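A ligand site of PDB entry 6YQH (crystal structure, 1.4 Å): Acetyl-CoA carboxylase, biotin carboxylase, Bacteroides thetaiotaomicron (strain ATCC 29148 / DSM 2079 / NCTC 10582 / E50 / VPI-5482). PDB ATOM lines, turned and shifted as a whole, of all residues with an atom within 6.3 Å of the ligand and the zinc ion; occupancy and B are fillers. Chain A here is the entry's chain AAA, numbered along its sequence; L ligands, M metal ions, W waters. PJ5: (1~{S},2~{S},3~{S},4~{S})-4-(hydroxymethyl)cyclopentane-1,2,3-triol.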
ATOM      1  N   TRP A  79      -0.653  -9.309  28.524  1.00  0.00           N
ATOM      2  CA  TRP A  79       0.589 -10.079  28.743  1.00  0.00           C
ATOM      3  C   TRP A  79       1.743  -9.094  28.987  1.00  0.00           C
ATOM      4  O   TRP A  79       2.818  -9.542  29.454  1.00  0.00           O
ATOM      5  CB  TRP A  79       0.869 -10.971  27.569  1.00  0.00           C
ATOM      6  CG  TRP A  79      -0.160 -12.025  27.253  1.00  0.00           C
ATOM      7  CD1 TRP A  79      -1.428 -12.172  27.748  1.00  0.00           C
ATOM      8  CD2 TRP A  79       0.039 -13.077  26.305  1.00  0.00           C
ATOM      9  NE1 TRP A  79      -2.047 -13.230  27.160  1.00  0.00           N
ATOM     10  CE2 TRP A  79      -1.157 -13.825  26.275  1.00  0.00           C
ATOM     11  CE3 TRP A  79       1.145 -13.535  25.564  1.00  0.00           C
ATOM     12  CZ2 TRP A  79      -1.325 -14.931  25.458  1.00  0.00           C
ATOM     13  CZ3 TRP A  79       0.984 -14.689  24.833  1.00  0.00           C
ATOM     14  CH2 TRP A  79      -0.238 -15.363  24.757  1.00  0.00           C
ATOM     15  N   LEU A  84       5.304 -11.058  30.222  1.00  0.00           N
ATOM     16  CA  LEU A  84       5.882 -11.079  28.855  1.00  0.00           C
ATOM     17  C   LEU A  84       6.181  -9.652  28.365  1.00  0.00           C
ATOM     18  O   LEU A  84       6.493  -9.442  27.193  1.00  0.00           O
ATOM     19  CB  LEU A  84       5.059 -11.919  27.880  1.00  0.00           C
ATOM     20  CG  LEU A  84       5.717 -13.245  27.488  1.00  0.00           C
ATOM     21  CD1 LEU A  84       4.739 -14.092  26.678  1.00  0.00           C
ATOM     22  CD2 LEU A  84       7.005 -13.016  26.680  1.00  0.00           C
ATOM     23  N   TRP A 160       8.549 -15.635  32.753  1.00  0.00           N
ATOM     24  CA  TRP A 160       7.742 -16.190  31.652  1.00  0.00           C
ATOM     25  C   TRP A 160       8.487 -16.110  30.319  1.00  0.00           C
ATOM     26  O   TRP A 160       8.719 -15.028  29.785  1.00  0.00           O
ATOM     27  CB  TRP A 160       6.423 -15.443  31.633  1.00  0.00           C
ATOM     28  CG  TRP A 160       5.364 -16.024  30.745  1.00  0.00           C
ATOM     29  CD1 TRP A 160       5.299 -17.253  30.151  1.00  0.00           C
ATOM     30  CD2 TRP A 160       4.175 -15.325  30.353  1.00  0.00           C
ATOM     31  NE1 TRP A 160       4.175 -17.339  29.398  1.00  0.00           N
ATOM     32  CE2 TRP A 160       3.425 -16.189  29.538  1.00  0.00           C
ATOM     33  CE3 TRP A 160       3.634 -14.083  30.674  1.00  0.00           C
ATOM     34  CZ2 TRP A 160       2.238 -15.792  28.942  1.00  0.00           C
ATOM     35  CZ3 TRP A 160       2.431 -13.718  30.147  1.00  0.00           C
ATOM     36  CH2 TRP A 160       1.732 -14.559  29.284  1.00  0.00           C
ATOM     37  N   VAL A 161       8.888 -17.274  29.795  1.00  0.00           N
ATOM     38  CA  VAL A 161       9.621 -17.475  28.506  1.00  0.00           C
ATOM     39  C   VAL A 161      10.543 -16.285  28.165  1.00  0.00           C
ATOM     40  O   VAL A 161      10.460 -15.706  27.079  1.00  0.00           O
ATOM     41  CB  VAL A 161       8.647 -17.840  27.375  1.00  0.00           C
ATOM     42  CG1 VAL A 161       8.023 -19.212  27.669  1.00  0.00           C
ATOM     43  CG2 VAL A 161       7.598 -16.776  27.091  1.00  0.00           C
ATOM     44  N   TYR A 164      12.262 -16.399  24.713  1.00  0.00           N
ATOM     45  CA  TYR A 164      11.299 -16.118  23.657  1.00  0.00           C
ATOM     46  C   TYR A 164      11.111 -14.615  23.518  1.00  0.00           C
ATOM     47  O   TYR A 164      10.992 -14.064  22.414  1.00  0.00           O
ATOM     48  CB  TYR A 164       9.964 -16.820  23.979  1.00  0.00           C
ATOM     49  CG  TYR A 164       8.799 -16.449  23.122  1.00  0.00           C
ATOM     50  CD1 TYR A 164       8.059 -15.321  23.366  1.00  0.00           C
ATOM     51  CD2 TYR A 164       8.383 -17.294  22.097  1.00  0.00           C
ATOM     52  CE1 TYR A 164       6.977 -14.973  22.574  1.00  0.00           C
ATOM     53  CE2 TYR A 164       7.254 -16.992  21.330  1.00  0.00           C
ATOM     54  CZ  TYR A 164       6.582 -15.809  21.548  1.00  0.00           C
ATOM     55  OH  TYR A 164       5.513 -15.498  20.767  1.00  0.00           O
ATOM     56  N   GLU A 215      10.909 -22.303  26.484  1.00  0.00           N
ATOM     57  CA  GLU A 215      10.621 -21.793  25.121  1.00  0.00           C
ATOM     58  C   GLU A 215      11.536 -20.617  24.806  1.00  0.00           C
ATOM     59  O   GLU A 215      11.616 -19.688  25.604  1.00  0.00           O
ATOM     60  CB  GLU A 215       9.131 -21.428  24.994  1.00  0.00           C
ATOM     61  CG  GLU A 215       8.778 -20.892  23.623  1.00  0.00           C
ATOM     62  CD  GLU A 215       7.349 -20.516  23.374  1.00  0.00           C
ATOM     63  OE1 GLU A 215       6.577 -20.465  24.322  1.00  0.00           O
ATOM     64  OE2 GLU A 215       7.038 -20.258  22.181  1.00  0.00           O
ATOM     65  N   HIS A 262       4.081 -28.497  22.550  1.00  0.00           N
ATOM     66  CA  HIS A 262       3.598 -27.149  22.216  1.00  0.00           C
ATOM     67  C   HIS A 262       4.126 -26.792  20.832  1.00  0.00           C
ATOM     68  O   HIS A 262       5.346 -26.817  20.624  1.00  0.00           O
ATOM     69  CB  HIS A 262       4.071 -26.154  23.278  1.00  0.00           C
ATOM     70  CG  HIS A 262       3.516 -24.789  23.035  1.00  0.00           C
ATOM     71  ND1 HIS A 262       4.183 -23.837  22.274  1.00  0.00           N
ATOM     72  CD2 HIS A 262       2.334 -24.223  23.373  1.00  0.00           C
ATOM     73  CE1 HIS A 262       3.428 -22.747  22.201  1.00  0.00           C
ATOM     74  NE2 HIS A 262       2.281 -22.966  22.862  1.00  0.00           N
ATOM     75  N   ALA A 263       3.251 -26.473  19.898  1.00  0.00           N
ATOM     76  CA  ALA A 263       3.636 -26.488  18.465  1.00  0.00           C
ATOM     77  C   ALA A 263       4.467 -25.243  18.102  1.00  0.00           C
ATOM     78  O   ALA A 263       5.527 -25.377  17.488  1.00  0.00           O
ATOM     79  CB  ALA A 263       2.392 -26.613  17.616  1.00  0.00           C
ATOM     80  N   ASN A 264       4.003 -24.036  18.448  1.00  0.00           N
ATOM     81  CA  ASN A 264       4.714 -22.810  18.065  1.00  0.00           C
ATOM     82  C   ASN A 264       6.061 -22.703  18.774  1.00  0.00           C
ATOM     83  O   ASN A 264       6.880 -21.915  18.340  1.00  0.00           O
ATOM     84  CB  ASN A 264       3.896 -21.540  18.231  1.00  0.00           C
ATOM     85  CG  ASN A 264       4.461 -20.379  17.442  1.00  0.00           C
ATOM     86  OD1 ASN A 264       4.541 -20.511  16.217  1.00  0.00           O
ATOM     87  ND2 ASN A 264       4.850 -19.321  18.138  1.00  0.00           N
ATOM     88  N   THR A 265       6.285 -23.443  19.851  1.00  0.00           N
ATOM     89  CA  THR A 265       7.633 -23.513  20.445  1.00  0.00           C
ATOM     90  C   THR A 265       8.632 -24.143  19.469  1.00  0.00           C
ATOM     91  O   THR A 265       9.782 -23.684  19.406  1.00  0.00           O
ATOM     92  CB  THR A 265       7.573 -24.295  21.756  1.00  0.00           C
ATOM     93  OG1 THR A 265       6.819 -23.568  22.716  1.00  0.00           O
ATOM     94  CG2 THR A 265       8.920 -24.655  22.346  1.00  0.00           C
ATOM     95  N   GLU A 318      -3.001 -25.168  21.144  1.00  0.00           N
ATOM     96  CA  GLU A 318      -1.572 -24.802  20.986  1.00  0.00           C
ATOM     97  C   GLU A 318      -0.665 -26.032  20.900  1.00  0.00           C
ATOM     98  O   GLU A 318       0.560 -25.792  20.740  1.00  0.00           O
ATOM     99  CB  GLU A 318      -1.016 -23.830  22.048  1.00  0.00           C
ATOM    100  CG  GLU A 318      -1.914 -22.626  22.253  1.00  0.00           C
ATOM    101  CD  GLU A 318      -1.332 -21.603  23.229  1.00  0.00           C
ATOM    102  OE1 GLU A 318      -0.176 -21.824  23.720  1.00  0.00           O
ATOM    103  OE2 GLU A 318      -2.091 -20.641  23.616  1.00  0.00           O
ATOM    104  N   GLU A 337      -3.751 -22.249  15.977  1.00  0.00           N
ATOM    105  CA  GLU A 337      -3.230 -20.979  16.430  1.00  0.00           C
ATOM    106  C   GLU A 337      -2.563 -20.239  15.270  1.00  0.00           C
ATOM    107  O   GLU A 337      -1.831 -20.864  14.489  1.00  0.00           O
ATOM    108  CB  GLU A 337      -2.242 -21.208  17.555  1.00  0.00           C
ATOM    109  CG  GLU A 337      -1.619 -19.983  18.083  1.00  0.00           C
ATOM    110  CD  GLU A 337      -0.496 -20.101  19.091  1.00  0.00           C
ATOM    111  OE1 GLU A 337       0.199 -19.089  19.246  1.00  0.00           O
ATOM    112  OE2 GLU A 337      -0.246 -21.180  19.658  1.00  0.00           O
ATOM    113  N   THR A 338      -2.741 -18.925  15.189  1.00  0.00           N
ATOM    114  CA  THR A 338      -2.238 -18.216  14.006  1.00  0.00           C
ATOM    115  C   THR A 338      -0.690 -18.164  13.961  1.00  0.00           C
ATOM    116  O   THR A 338      -0.127 -18.337  12.866  1.00  0.00           O
ATOM    117  CB  THR A 338      -2.874 -16.838  13.899  1.00  0.00           C
ATOM    118  OG1 THR A 338      -4.248 -16.898  14.264  1.00  0.00           O
ATOM    119  CG2 THR A 338      -2.731 -16.272  12.510  1.00  0.00           C
ATOM    120  N   CYS A 339      -0.031 -17.941  15.088  1.00  0.00           N
ATOM    121  CA  CYS A 339       1.452 -17.924  15.104  1.00  0.00           C
ATOM    122  C   CYS A 339       1.990 -19.118  14.322  1.00  0.00           C
ATOM    123  O   CYS A 339       2.970 -18.952  13.578  1.00  0.00           O
ATOM    124  CB  CYS A 339       2.044 -18.008  16.496  1.00  0.00           C
ATOM    125  SG  CYS A 339       1.905 -16.496  17.497  1.00  0.00           S
ATOM    126  N   ASN A 340       1.408 -20.292  14.531  1.00  0.00           N
ATOM    127  CA  ASN A 340       2.019 -21.509  13.997  1.00  0.00           C
ATOM    128  C   ASN A 340       2.064 -21.383  12.465  1.00  0.00           C
ATOM    129  O   ASN A 340       3.018 -21.891  11.854  1.00  0.00           O
ATOM    130  CB  ASN A 340       1.219 -22.740  14.404  1.00  0.00           C
ATOM    131  CG  ASN A 340       0.883 -22.864  15.857  1.00  0.00           C
ATOM    132  OD1 ASN A 340       0.882 -21.893  16.601  1.00  0.00           O
ATOM    133  ND2 ASN A 340       0.518 -24.061  16.238  1.00  0.00           N
ATOM    134  N   TYR A 393      -6.406 -15.315  17.405  1.00  0.00           N
ATOM    135  CA  TYR A 393      -5.485 -16.265  18.065  1.00  0.00           C
ATOM    136  C   TYR A 393      -5.872 -17.679  17.619  1.00  0.00           C
ATOM    137  O   TYR A 393      -5.040 -18.386  17.070  1.00  0.00           O
ATOM    138  CB  TYR A 393      -5.584 -16.069  19.573  1.00  0.00           C
ATOM    139  CG  TYR A 393      -4.482 -16.647  20.449  1.00  0.00           C
ATOM    140  CD1 TYR A 393      -4.265 -17.996  20.504  1.00  0.00           C
ATOM    141  CD2 TYR A 393      -3.678 -15.833  21.217  1.00  0.00           C
ATOM    142  CE1 TYR A 393      -3.296 -18.524  21.339  1.00  0.00           C
ATOM    143  CE2 TYR A 393      -2.745 -16.339  22.101  1.00  0.00           C
ATOM    144  CZ  TYR A 393      -2.555 -17.695  22.144  1.00  0.00           C
ATOM    145  OH  TYR A 393      -1.587 -18.161  23.025  1.00  0.00           O
ATOM    146  N   TRP A 413      -1.128 -10.522  22.966  1.00  0.00           N
ATOM    147  CA  TRP A 413      -0.893 -11.966  22.748  1.00  0.00           C
ATOM    148  C   TRP A 413       0.250 -12.242  21.769  1.00  0.00           C
ATOM    149  O   TRP A 413       0.550 -11.427  20.903  1.00  0.00           O
ATOM    150  CB  TRP A 413      -2.157 -12.604  22.220  1.00  0.00           C
ATOM    151  CG  TRP A 413      -3.446 -12.137  22.760  1.00  0.00           C
ATOM    152  CD1 TRP A 413      -3.758 -11.819  24.072  1.00  0.00           C
ATOM    153  CD2 TRP A 413      -4.669 -12.058  22.011  1.00  0.00           C
ATOM    154  NE1 TRP A 413      -5.076 -11.420  24.142  1.00  0.00           N
ATOM    155  CE2 TRP A 413      -5.650 -11.552  22.905  1.00  0.00           C
ATOM    156  CE3 TRP A 413      -5.010 -12.215  20.683  1.00  0.00           C
ATOM    157  CZ2 TRP A 413      -6.943 -11.288  22.496  1.00  0.00           C
ATOM    158  CZ3 TRP A 413      -6.302 -11.997  20.282  1.00  0.00           C
ATOM    159  CH2 TRP A 413      -7.262 -11.527  21.182  1.00  0.00           C
ATOM    160  N   CYS A 414       0.776 -13.459  21.835  1.00  0.00           N
ATOM    161  CA  CYS A 414       1.715 -13.942  20.798  1.00  0.00           C
ATOM    162  C   CYS A 414       1.107 -13.714  19.409  1.00  0.00           C
ATOM    163  O   CYS A 414       1.831 -13.287  18.486  1.00  0.00           O
ATOM    164  CB  CYS A 414       2.174 -15.372  21.007  1.00  0.00           C
ATOM    165  SG  CYS A 414       0.781 -16.544  21.232  1.00  0.00           S
ATOM    166  N   CYS A 415      -0.143 -14.062  19.205  1.00  0.00           N
ATOM    167  CA  CYS A 415      -0.827 -13.923  17.923  1.00  0.00           C
ATOM    168  C   CYS A 415      -1.094 -12.473  17.540  1.00  0.00           C
ATOM    169  O   CYS A 415      -1.346 -12.225  16.346  1.00  0.00           O
ATOM    170  CB  CYS A 415      -2.100 -14.777  17.881  1.00  0.00           C
ATOM    171  SG  CYS A 415      -1.852 -16.576  17.908  1.00  0.00           S
ATOM    172  N   VAL A 416      -1.004 -11.507  18.462  1.00  0.00           N
ATOM    173  CA  VAL A 416      -0.989 -10.094  18.058  1.00  0.00           C
ATOM    174  C   VAL A 416       0.384  -9.800  17.468  1.00  0.00           C
ATOM    175  O   VAL A 416       0.467  -9.108  16.461  1.00  0.00           O
ATOM    176  CB  VAL A 416      -1.331  -9.167  19.215  1.00  0.00           C
ATOM    177  CG1 VAL A 416      -1.051  -7.710  18.903  1.00  0.00           C
ATOM    178  CG2 VAL A 416      -2.747  -9.327  19.682  1.00  0.00           C
ATOM    179  N   SER A 418       2.699 -11.752  16.007  1.00  0.00           N
ATOM    180  CA  SER A 418       2.797 -12.331  14.640  1.00  0.00           C
ATOM    181  C   SER A 418       1.763 -11.695  13.697  1.00  0.00           C
ATOM    182  O   SER A 418       2.071 -11.477  12.520  1.00  0.00           O
ATOM    183  CB  SER A 418       2.698 -13.841  14.680  1.00  0.00           C
ATOM    184  OG  SER A 418       1.490 -14.248  15.282  1.00  0.00           O
ATOM    185  N   GLN A 686       0.914 -24.612  28.915  1.00  0.00           N
ATOM    186  CA  GLN A 686       1.518 -23.334  29.332  1.00  0.00           C
ATOM    187  C   GLN A 686       0.525 -22.181  29.376  1.00  0.00           C
ATOM    188  O   GLN A 686       0.565 -21.426  30.342  1.00  0.00           O
ATOM    189  CB  GLN A 686       2.783 -23.022  28.535  1.00  0.00           C
ATOM    190  CG  GLN A 686       2.601 -22.828  27.032  1.00  0.00           C
ATOM    191  CD  GLN A 686       3.976 -22.627  26.408  1.00  0.00           C
ATOM    192  OE1 GLN A 686       4.861 -23.450  26.599  1.00  0.00           O
ATOM    193  NE2 GLN A 686       4.140 -21.608  25.557  1.00  0.00           N
ATOM    194  N   GLN A 687      -0.269 -21.956  28.340  1.00  0.00           N
ATOM    195  CA  GLN A 687      -1.054 -20.720  28.287  1.00  0.00           C
ATOM    196  C   GLN A 687      -2.209 -20.819  29.275  1.00  0.00           C
ATOM    197  O   GLN A 687      -2.458 -19.856  29.997  1.00  0.00           O
ATOM    198  CB  GLN A 687      -1.428 -20.273  26.886  1.00  0.00           C
ATOM    199  CG  GLN A 687      -1.928 -18.841  26.935  1.00  0.00           C
ATOM    200  CD  GLN A 687      -0.934 -17.822  27.484  1.00  0.00           C
ATOM    201  OE1 GLN A 687      -1.309 -16.858  28.250  1.00  0.00           O
ATOM    202  NE2 GLN A 687       0.319 -18.070  27.209  1.00  0.00           N
HETATM  203  O1' PJ5 L   1       2.243 -20.252  20.881  1.00  0.00           O
HETATM  204  C1' PJ5 L   1       2.534 -18.862  20.926  1.00  0.00           C
HETATM  205  C6' PJ5 L   1       1.585 -18.068  21.840  1.00  0.00           C
HETATM  206  C2' PJ5 L   1       3.912 -18.712  21.553  1.00  0.00           C
HETATM  207  O2' PJ5 L   1       4.902 -19.560  21.014  1.00  0.00           O
HETATM  208  C3' PJ5 L   1       3.655 -18.852  23.043  1.00  0.00           C
HETATM  209  O3' PJ5 L   1       4.752 -18.370  23.900  1.00  0.00           O
HETATM  210  C4' PJ5 L   1       2.374 -18.056  23.232  1.00  0.00           C
HETATM  211  C5' PJ5 L   1       1.522 -18.642  24.357  1.00  0.00           C
HETATM  212  O5' PJ5 L   1       1.682 -19.974  24.666  1.00  0.00           O
HETATM  213 ZN    ZN M   1       0.117 -17.121  18.893  1.00  0.00          ZN
HETATM  214  O   HOH W   1       4.433 -18.391  26.578  1.00  0.00           O
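Four residues have an atom within 4 Å of the zinc ion: Glu 337, Cys 339, Cys 414 and Cys 415.
The nearest printed residue that does not touch the zinc ion is Tyr 393 (4.2 Å).
OE1 of Glu 337 binds the zinc ion, at 2.0 Å.
The zinc ion is bound by SG of Cys 415, 2.3 Å away.
SG of Cys 339 binds the zinc ion, 2.4 Å away.
The zinc ion is bound by SG of Cys 414, 2.5 Å away.
The zinc ion has four donor atoms within binding distance.
OE2 of Glu 318 lies within hydrogen-bond range of OH of Tyr 393 (2.6 Å).
The side-chain carboxylate (OE1) of Glu 215 lies within hydrogen-bond range of the side-chain amide nitrogen (NE2) of Gln 686, 3.0 Å away.
The side-chain sulfur of Cys 414 sits close to the side-chain hydroxyl of Tyr 393.
The side-chain sulfur (SG) of Cys 415 sits close to the backbone NH (N) of Thr 338.
OE2 of Glu 215 sits close to OG1 of Thr 265 (3.4 Å).
The backbone carbonyl oxygen (O) of Glu 318 sits at hydrogen-bond distance from the backbone NH (N) of Ala 263, 2.9 Å away.
O of Glu 215 sits at hydrogen-bond distance from N of Tyr 164, at 3.5 Å.
The side-chain sulfur (SG) of Cys 339 lies close to the side-chain hydroxyl (OG) of Ser 418 (3.2 Å).
Water W1 lies within hydrogen-bond range of O3' of the ligand, NE1 of Trp 160 and NE2 of Gln 686.
Residues that only touch the ligand: Trp 79 (3.7 Å), Tyr 164 (3.5 Å) and Tyr 393 (3.4 Å).
Hydrophobic or aromatic side chains within 4 Å of the ligand: Trp 79, Tyr 164 and His 262.
Within 4 Å of the ligand: Trp 79, Tyr 164, Glu 215, His 262, Asn 264, Glu 318, Glu 337, Tyr 393, Cys 414, Gln 686 and Gln 687.
The nearest printed residue that does not touch the ligand is Cys 339 (4.2 Å).
O5' of the ligand sits close to NE2 of Gln 687 (3.5 Å).
ND2 of Asn 264 sits at hydrogen-bond distance from O2' of the ligand (2.9 Å).
An oxygen (O2') of the ligand lies within hydrogen-bond range of the side-chain carboxylate of Glu 215 (2.5 Å).
NE2 of Gln 686 sits at hydrogen-bond distance from O5' of the ligand (3.1 Å).
The side-chain carboxylate (OE2) of Glu 337 lies within hydrogen-bond range of an oxygen (O1') of the ligand (2.9 Å).
The side-chain carboxylate (OE1) of Glu 318 lies within hydrogen-bond range of an oxygen (O5') of the ligand, at 2.8 Å.
An oxygen (O1') of the ligand lies close to a ring nitrogen (NE2) of His 262 (3.4 Å).
The side-chain sulfur of Cys 414 is covalently linked to a carbon (C6') of the ligand (1.8 Å).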
